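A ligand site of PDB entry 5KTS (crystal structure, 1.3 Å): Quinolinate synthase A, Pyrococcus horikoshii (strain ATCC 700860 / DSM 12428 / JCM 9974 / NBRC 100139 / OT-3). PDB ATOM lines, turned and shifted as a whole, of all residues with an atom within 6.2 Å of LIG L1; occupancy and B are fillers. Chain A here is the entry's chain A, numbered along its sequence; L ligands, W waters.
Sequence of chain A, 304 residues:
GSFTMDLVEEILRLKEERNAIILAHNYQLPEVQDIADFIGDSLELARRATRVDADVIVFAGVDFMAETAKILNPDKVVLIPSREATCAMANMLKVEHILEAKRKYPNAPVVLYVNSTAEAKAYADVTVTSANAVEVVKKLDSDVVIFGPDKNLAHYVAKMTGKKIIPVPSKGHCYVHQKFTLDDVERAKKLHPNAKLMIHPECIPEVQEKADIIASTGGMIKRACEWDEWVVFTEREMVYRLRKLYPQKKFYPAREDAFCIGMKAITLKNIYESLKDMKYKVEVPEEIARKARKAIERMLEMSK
N of Thr 217 lies within hydrogen-bond range of O2 of LIG L1. OG1 of Thr 217 sits at hydrogen-bond distance from O1 of LIG L1, at 2.5 Å. O2 of LIG L1 lies within hydrogen-bond range of NE2 of His 200. A ring nitrogen (NE2) of His 25 lies within hydrogen-bond range of an oxygen (O1) of LIG L1, at 2.9 Å. The backbone NH (N) of Ser 130 sits at hydrogen-bond distance from an oxygen (O4) of LIG L1. N of Ser 42 sits at hydrogen-bond distance from O3 of LIG L1 (3.1 Å). An oxygen (O4) of LIG L1 sits close to the side-chain hydroxyl (OH) of Tyr 113, 3.3 Å away. ND2 of Asn 115 lies close to S2 of LG2 L2.
The side-chain hydroxyl (OG1) of Thr 217 is in hydrogen-bond range of the side-chain amide nitrogen (ND2) of Asn 26 (2.9 Å). ND1 of His 25 lies within hydrogen-bond range of N of Tyr 27 (2.9 Å). The side-chain hydroxyl (OH) of Tyr 113 is in hydrogen-bond range of the side-chain hydroxyl (OG) of Ser 130 (2.5 Å). The side-chain carboxylate of Glu 202 sits at hydrogen-bond distance from the side-chain hydroxyl of Tyr 113 (2.5 Å). The side-chain hydroxyl (OG) of Ser 216 is in hydrogen-bond range of the side-chain carboxylate (OD2) of Asp 41 (2.7 Å). The side-chain carboxylate (OD1) of Asp 41 is in hydrogen-bond range of the backbone NH (N) of Leu 43. The side-chain hydroxyl (OG) of Ser 216 sits at hydrogen-bond distance from the backbone NH (N) of Gly 218. OE1 of Glu 202 lies within hydrogen-bond range of ND1 of His 177 (3.2 Å).
Merely in contact with LIG L1: Thr 129, Tyr 27, Asp 41, Ser 216 and Glu 202. Within 4 Å of LIG L1: His 25, Tyr 27, Asp 41, Ser 42, Tyr 113, Thr 129, Ser 130, His 200, Glu 202, Ser 216 and Thr 217.
Water W1 lies within hydrogen-bond range of O3 of LIG L1 (2.5 Å), OG1 of Thr 129 (2.7 Å), OD2 of Asp 41 (2.8 Å) and N of Leu 43 (3.0 Å). Water W2 lies within hydrogen-bond range of the side-chain amide oxygen of Asn 115 (2.5 Å), an oxygen (O4) of LIG L1 (2.8 Å) and the side-chain hydroxyl of Ser 42 (3.2 Å).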
ATOM      1  N   HIS A  25       8.010  -3.262  25.493  1.00  0.00           N
ATOM      2  CA  HIS A  25       9.235  -3.613  26.180  1.00  0.00           C
ATOM      3  C   HIS A  25       9.197  -5.089  26.587  1.00  0.00           C
ATOM      4  O   HIS A  25       8.141  -5.696  26.751  1.00  0.00           O
ATOM      5  CB  HIS A  25       9.430  -2.742  27.412  1.00  0.00           C
ATOM      6  CG  HIS A  25      10.757  -2.925  28.050  1.00  0.00           C
ATOM      7  ND1 HIS A  25      10.949  -3.789  29.116  1.00  0.00           N
ATOM      8  CD2 HIS A  25      11.978  -2.427  27.745  1.00  0.00           C
ATOM      9  CE1 HIS A  25      12.227  -3.797  29.450  1.00  0.00           C
ATOM     10  NE2 HIS A  25      12.882  -2.984  28.625  1.00  0.00           N
ATOM     11  N   ASN A  26      10.394  -5.662  26.750  1.00  0.00           N
ATOM     12  CA  ASN A  26      10.570  -7.043  27.175  1.00  0.00           C
ATOM     13  C   ASN A  26       9.934  -7.379  28.520  1.00  0.00           C
ATOM     14  O   ASN A  26       9.756  -8.568  28.820  1.00  0.00           O
ATOM     15  CB  ASN A  26      12.076  -7.380  27.231  1.00  0.00           C
ATOM     16  CG  ASN A  26      12.695  -7.504  25.859  1.00  0.00           C
ATOM     17  OD1 ASN A  26      12.069  -8.043  24.945  1.00  0.00           O
ATOM     18  ND2 ASN A  26      13.923  -7.032  25.719  1.00  0.00           N
ATOM     19  N   TYR A  27       9.595  -6.388  29.361  1.00  0.00           N
ATOM     20  CA  TYR A  27       8.988  -6.664  30.659  1.00  0.00           C
ATOM     21  C   TYR A  27       7.469  -6.639  30.609  1.00  0.00           C
ATOM     22  O   TYR A  27       6.826  -6.755  31.652  1.00  0.00           O
ATOM     23  CB  TYR A  27       9.460  -5.653  31.719  1.00  0.00           C
ATOM     24  CG  TYR A  27      10.956  -5.625  31.992  1.00  0.00           C
ATOM     25  CD1 TYR A  27      11.783  -6.683  31.617  1.00  0.00           C
ATOM     26  CD2 TYR A  27      11.539  -4.528  32.633  1.00  0.00           C
ATOM     27  CE1 TYR A  27      13.160  -6.646  31.871  1.00  0.00           C
ATOM     28  CE2 TYR A  27      12.899  -4.469  32.871  1.00  0.00           C
ATOM     29  CZ  TYR A  27      13.713  -5.530  32.492  1.00  0.00           C
ATOM     30  OH  TYR A  27      15.065  -5.449  32.764  1.00  0.00           O
ATOM     31  N   GLY A  40      11.310  -5.168  22.437  1.00  0.00           N
ATOM     32  CA  GLY A  40      12.742  -4.997  22.577  1.00  0.00           C
ATOM     33  C   GLY A  40      13.127  -4.270  23.857  1.00  0.00           C
ATOM     34  O   GLY A  40      12.292  -3.972  24.706  1.00  0.00           O
ATOM     35  N   ASP A  41      14.448  -4.008  23.983  1.00  0.00           N
ATOM     36  CA  ASP A  41      15.021  -3.274  25.096  1.00  0.00           C
ATOM     37  C   ASP A  41      14.978  -1.779  24.785  1.00  0.00           C
ATOM     38  O   ASP A  41      14.436  -1.362  23.767  1.00  0.00           O
ATOM     39  CB  ASP A  41      16.420  -3.809  25.479  1.00  0.00           C
ATOM     40  CG  ASP A  41      17.526  -3.400  24.500  1.00  0.00           C
ATOM     41  OD1 ASP A  41      17.246  -2.804  23.450  1.00  0.00           O
ATOM     42  OD2 ASP A  41      18.718  -3.694  24.812  1.00  0.00           O
ATOM     43  N   SER A  42      15.547  -0.967  25.678  1.00  0.00           N
ATOM     44  CA  SER A  42      15.407   0.479  25.521  1.00  0.00           C
ATOM     45  C   SER A  42      16.091   0.975  24.257  1.00  0.00           C
ATOM     46  O   SER A  42      15.523   1.813  23.531  1.00  0.00           O
ATOM     47  CB  SER A  42      15.925   1.204  26.765  1.00  0.00           C
ATOM     48  OG  SER A  42      15.069   1.015  27.887  1.00  0.00           O
ATOM     49  N   LEU A  43      17.289   0.462  23.954  1.00  0.00           N
ATOM     50  CA  LEU A  43      17.994   0.900  22.747  1.00  0.00           C
ATOM     51  C   LEU A  43      17.271   0.444  21.491  1.00  0.00           C
ATOM     52  O   LEU A  43      17.158   1.213  20.521  1.00  0.00           O
ATOM     53  CB  LEU A  43      19.428   0.375  22.769  1.00  0.00           C
ATOM     54  CG  LEU A  43      20.280   0.717  21.536  1.00  0.00           C
ATOM     55  CD1 LEU A  43      20.280   2.221  21.251  1.00  0.00           C
ATOM     56  CD2 LEU A  43      21.691   0.216  21.736  1.00  0.00           C
ATOM     57  N   MET A  65       9.725   5.869  28.092  1.00  0.00           N
ATOM     58  CA  MET A  65       9.932   5.185  26.812  1.00  0.00           C
ATOM     59  C   MET A  65       9.003   5.741  25.748  1.00  0.00           C
ATOM     60  O   MET A  65       9.431   5.977  24.611  1.00  0.00           O
ATOM     61  CB  MET A  65       9.679   3.690  26.974  1.00  0.00           C
ATOM     62  CG  MET A  65      10.648   3.029  27.902  1.00  0.00           C
ATOM     63  SD  MET A  65      10.257   1.292  28.117  1.00  0.00           S
ATOM     64  CE  MET A  65      11.636   0.860  29.205  1.00  0.00           C
ATOM     65  N   TYR A 113      21.103   8.075  31.102  1.00  0.00           N
ATOM     66  CA  TYR A 113      20.438   6.817  30.828  1.00  0.00           C
ATOM     67  C   TYR A 113      19.070   7.163  30.281  1.00  0.00           C
ATOM     68  O   TYR A 113      18.435   8.127  30.729  1.00  0.00           O
ATOM     69  CB  TYR A 113      20.301   6.069  32.160  1.00  0.00           C
ATOM     70  CG  TYR A 113      20.066   4.576  32.120  1.00  0.00           C
ATOM     71  CD1 TYR A 113      20.302   3.824  30.974  1.00  0.00           C
ATOM     72  CD2 TYR A 113      19.633   3.910  33.258  1.00  0.00           C
ATOM     73  CE1 TYR A 113      20.077   2.451  30.970  1.00  0.00           C
ATOM     74  CE2 TYR A 113      19.423   2.564  33.260  1.00  0.00           C
ATOM     75  CZ  TYR A 113      19.643   1.837  32.120  1.00  0.00           C
ATOM     76  OH  TYR A 113      19.417   0.481  32.155  1.00  0.00           O
ATOM     77  N   VAL A 114      18.639   6.400  29.275  1.00  0.00           N
ATOM     78  CA  VAL A 114      17.324   6.628  28.682  1.00  0.00           C
ATOM     79  C   VAL A 114      16.231   6.541  29.743  1.00  0.00           C
ATOM     80  O   VAL A 114      15.185   7.183  29.627  1.00  0.00           O
ATOM     81  CB  VAL A 114      17.108   5.712  27.459  1.00  0.00           C
ATOM     82  CG1 VAL A 114      15.658   5.764  26.975  1.00  0.00           C
ATOM     83  CG2 VAL A 114      18.047   6.125  26.326  1.00  0.00           C
ATOM     84  N   ASN A 115      16.483   5.808  30.826  1.00  0.00           N
ATOM     85  CA  ASN A 115      15.583   5.814  31.976  1.00  0.00           C
ATOM     86  C   ASN A 115      15.688   7.173  32.657  1.00  0.00           C
ATOM     87  O   ASN A 115      16.306   7.336  33.710  1.00  0.00           O
ATOM     88  CB  ASN A 115      15.925   4.697  32.966  1.00  0.00           C
ATOM     89  CG  ASN A 115      15.905   3.316  32.320  1.00  0.00           C
ATOM     90  OD1 ASN A 115      16.376   3.128  31.203  1.00  0.00           O
ATOM     91  ND2 ASN A 115      15.372   2.332  33.047  1.00  0.00           N
ATOM     92  N   VAL A 128      22.237   7.179  26.828  1.00  0.00           N
ATOM     93  CA  VAL A 128      22.732   5.816  26.787  1.00  0.00           C
ATOM     94  C   VAL A 128      21.656   4.864  27.295  1.00  0.00           C
ATOM     95  O   VAL A 128      20.694   5.270  27.951  1.00  0.00           O
ATOM     96  CB  VAL A 128      24.016   5.586  27.623  1.00  0.00           C
ATOM     97  CG1 VAL A 128      25.187   6.363  27.054  1.00  0.00           C
ATOM     98  CG2 VAL A 128      23.773   5.933  29.097  1.00  0.00           C
ATOM     99  N   THR A 129      21.843   3.595  26.992  1.00  0.00           N
ATOM    100  CA  THR A 129      21.072   2.535  27.615  1.00  0.00           C
ATOM    101  C   THR A 129      22.068   1.532  28.184  1.00  0.00           C
ATOM    102  O   THR A 129      23.280   1.682  28.043  1.00  0.00           O
ATOM    103  CB  THR A 129      20.140   1.836  26.615  1.00  0.00           C
ATOM    104  OG1 THR A 129      20.901   0.953  25.803  1.00  0.00           O
ATOM    105  CG2 THR A 129      19.402   2.843  25.735  1.00  0.00           C
ATOM    106  N   SER A 130      21.536   0.485  28.810  1.00  0.00           N
ATOM    107  CA  SER A 130      22.412  -0.558  29.356  1.00  0.00           C
ATOM    108  C   SER A 130      23.215  -1.244  28.248  1.00  0.00           C
ATOM    109  O   SER A 130      24.303  -1.765  28.517  1.00  0.00           O
ATOM    110  CB  SER A 130      21.591  -1.576  30.149  1.00  0.00           C
ATOM    111  OG  SER A 130      21.274  -1.083  31.449  1.00  0.00           O
ATOM    112  N   ALA A 131      22.725  -1.234  27.014  1.00  0.00           N
ATOM    113  CA  ALA A 131      23.395  -1.934  25.926  1.00  0.00           C
ATOM    114  C   ALA A 131      24.599  -1.177  25.390  1.00  0.00           C
ATOM    115  O   ALA A 131      25.529  -1.803  24.892  1.00  0.00           O
ATOM    116  CB  ALA A 131      22.399  -2.228  24.800  1.00  0.00           C
ATOM    117  N   LEU A 153      24.426   0.729  37.194  1.00  0.00           N
ATOM    118  CA  LEU A 153      24.965   0.851  35.849  1.00  0.00           C
ATOM    119  C   LEU A 153      26.206   1.749  35.829  1.00  0.00           C
ATOM    120  O   LEU A 153      27.174   1.470  35.123  1.00  0.00           O
ATOM    121  CB  LEU A 153      23.903   1.378  34.891  1.00  0.00           C
ATOM    122  CG  LEU A 153      24.363   1.593  33.429  1.00  0.00           C
ATOM    123  CD1 LEU A 153      24.891   0.305  32.814  1.00  0.00           C
ATOM    124  CD2 LEU A 153      23.207   2.166  32.610  1.00  0.00           C
ATOM    125  N   HIS A 177      15.704  -4.472  40.229  1.00  0.00           N
ATOM    126  CA  HIS A 177      17.015  -5.107  40.128  1.00  0.00           C
ATOM    127  C   HIS A 177      17.779  -5.094  41.446  1.00  0.00           C
ATOM    128  O   HIS A 177      18.626  -5.965  41.676  1.00  0.00           O
ATOM    129  CB  HIS A 177      17.824  -4.474  39.012  1.00  0.00           C
ATOM    130  CG  HIS A 177      17.304  -4.826  37.660  1.00  0.00           C
ATOM    131  ND1 HIS A 177      16.397  -4.035  36.984  1.00  0.00           N
ATOM    132  CD2 HIS A 177      17.495  -5.925  36.893  1.00  0.00           C
ATOM    133  CE1 HIS A 177      16.096  -4.623  35.833  1.00  0.00           C
ATOM    134  NE2 HIS A 177      16.744  -5.767  35.755  1.00  0.00           N
ATOM    135  N   HIS A 200      21.611  -8.351  34.701  1.00  0.00           N
ATOM    136  CA  HIS A 200      21.460  -6.995  34.216  1.00  0.00           C
ATOM    137  C   HIS A 200      22.403  -6.058  34.983  1.00  0.00           C
ATOM    138  O   HIS A 200      22.575  -6.224  36.193  1.00  0.00           O
ATOM    139  CB  HIS A 200      20.009  -6.545  34.426  1.00  0.00           C
ATOM    140  CG  HIS A 200      19.625  -5.395  33.568  1.00  0.00           C
ATOM    141  ND1 HIS A 200      19.937  -4.089  33.880  1.00  0.00           N
ATOM    142  CD2 HIS A 200      18.957  -5.351  32.383  1.00  0.00           C
ATOM    143  CE1 HIS A 200      19.492  -3.290  32.920  1.00  0.00           C
ATOM    144  NE2 HIS A 200      18.888  -4.030  32.006  1.00  0.00           N
ATOM    145  N   GLU A 202      21.853  -3.204  36.080  1.00  0.00           N
ATOM    146  CA  GLU A 202      21.148  -2.493  37.149  1.00  0.00           C
ATOM    147  C   GLU A 202      21.187  -3.257  38.469  1.00  0.00           C
ATOM    148  O   GLU A 202      20.799  -2.693  39.501  1.00  0.00           O
ATOM    149  CB  GLU A 202      19.703  -2.164  36.739  1.00  0.00           C
ATOM    150  CG  GLU A 202      19.608  -1.141  35.602  1.00  0.00           C
ATOM    151  CD  GLU A 202      18.184  -0.815  35.178  1.00  0.00           C
ATOM    152  OE1 GLU A 202      17.234  -1.138  35.932  1.00  0.00           O
ATOM    153  OE2 GLU A 202      17.999  -0.231  34.080  1.00  0.00           O
ATOM    154  N   ALA A 215      24.471  -7.932  30.753  1.00  0.00           N
ATOM    155  CA  ALA A 215      23.870  -7.459  29.513  1.00  0.00           C
ATOM    156  C   ALA A 215      22.539  -6.777  29.807  1.00  0.00           C
ATOM    157  O   ALA A 215      21.867  -7.101  30.795  1.00  0.00           O
ATOM    158  CB  ALA A 215      23.645  -8.615  28.537  1.00  0.00           C
ATOM    159  N   SER A 216      22.156  -5.854  28.914  1.00  0.00           N
ATOM    160  CA  SER A 216      20.769  -5.405  28.851  1.00  0.00           C
ATOM    161  C   SER A 216      19.891  -6.575  28.428  1.00  0.00           C
ATOM    162  O   SER A 216      20.384  -7.642  28.032  1.00  0.00           O
ATOM    163  CB  SER A 216      20.618  -4.294  27.817  1.00  0.00           C
ATOM    164  OG  SER A 216      20.550  -4.820  26.506  1.00  0.00           O
ATOM    165  N   THR A 217      18.576  -6.376  28.486  1.00  0.00           N
ATOM    166  CA  THR A 217      17.698  -7.449  28.035  1.00  0.00           C
ATOM    167  C   THR A 217      17.932  -7.754  26.553  1.00  0.00           C
ATOM    168  O   THR A 217      17.865  -8.913  26.143  1.00  0.00           O
ATOM    169  CB  THR A 217      16.227  -7.126  28.314  1.00  0.00           C
ATOM    170  OG1 THR A 217      15.836  -5.957  27.584  1.00  0.00           O
ATOM    171  CG2 THR A 217      15.981  -6.899  29.800  1.00  0.00           C
ATOM    172  N   GLY A 218      18.274  -6.737  25.754  1.00  0.00           N
ATOM    173  CA  GLY A 218      18.610  -7.007  24.358  1.00  0.00           C
ATOM    174  C   GLY A 218      19.876  -7.822  24.232  1.00  0.00           C
ATOM    175  O   GLY A 218      19.948  -8.754  23.415  1.00  0.00           O
ATOM    176  N   THR A 234      16.857 -10.505  35.960  1.00  0.00           N
ATOM    177  CA  THR A 234      16.168  -9.280  35.592  1.00  0.00           C
ATOM    178  C   THR A 234      14.684  -9.478  35.882  1.00  0.00           C
ATOM    179  O   THR A 234      14.279 -10.484  36.464  1.00  0.00           O
ATOM    180  CB  THR A 234      16.521  -8.835  34.163  1.00  0.00           C
ATOM    181  OG1 THR A 234      16.048  -7.514  33.952  1.00  0.00           O
ATOM    182  CG2 THR A 234      15.932  -9.761  33.112  1.00  0.00           C
HETATM  183  O1  LIG L   1      15.653  -3.676  28.689  1.00  0.00           O
HETATM  184  C1  LIG L   1      16.662  -3.351  29.505  1.00  0.00           C
HETATM  185  O2  LIG L   1      17.723  -3.956  29.496  1.00  0.00           O
HETATM  186  C2  LIG L   1      16.473  -2.213  30.407  1.00  0.00           C
HETATM  187  C3  LIG L   1      15.684  -2.424  31.671  1.00  0.00           C
HETATM  188  C4  LIG L   1      16.987  -1.006  30.114  1.00  0.00           C
HETATM  189  C5  LIG L   1      17.798  -0.719  28.910  1.00  0.00           C
HETATM  190  O3  LIG L   1      17.719  -1.368  27.878  1.00  0.00           O
HETATM  191  O4  LIG L   1      18.670   0.281  28.982  1.00  0.00           O
HETATM  192 FE1  LG2 L   2      12.178   1.578  35.911  1.00  0.00          FE
HETATM  193 FE2  LG2 L   2      10.630  -0.619  36.175  1.00  0.00          FE
HETATM  194 FE3  LG2 L   2      13.230  -0.647  37.008  1.00  0.00          FE
HETATM  195 FE4  LG2 L   2      12.592  -0.438  34.340  1.00  0.00          FE
HETATM  196  S1  LG2 L   2      12.185  -2.220  35.752  1.00  0.00           S
HETATM  197  S2  LG2 L   2      14.233   0.697  35.518  1.00  0.00           S
HETATM  198  S3  LG2 L   2      10.679   0.802  34.424  1.00  0.00           S
HETATM  199  S4  LG2 L   2      11.553   0.633  37.884  1.00  0.00           S
HETATM  200  O   HOH W   1      19.107  -1.109  25.791  1.00  0.00           O
HETATM  201  O   HOH W   2      17.480   2.833  28.969  1.00  0.00           O
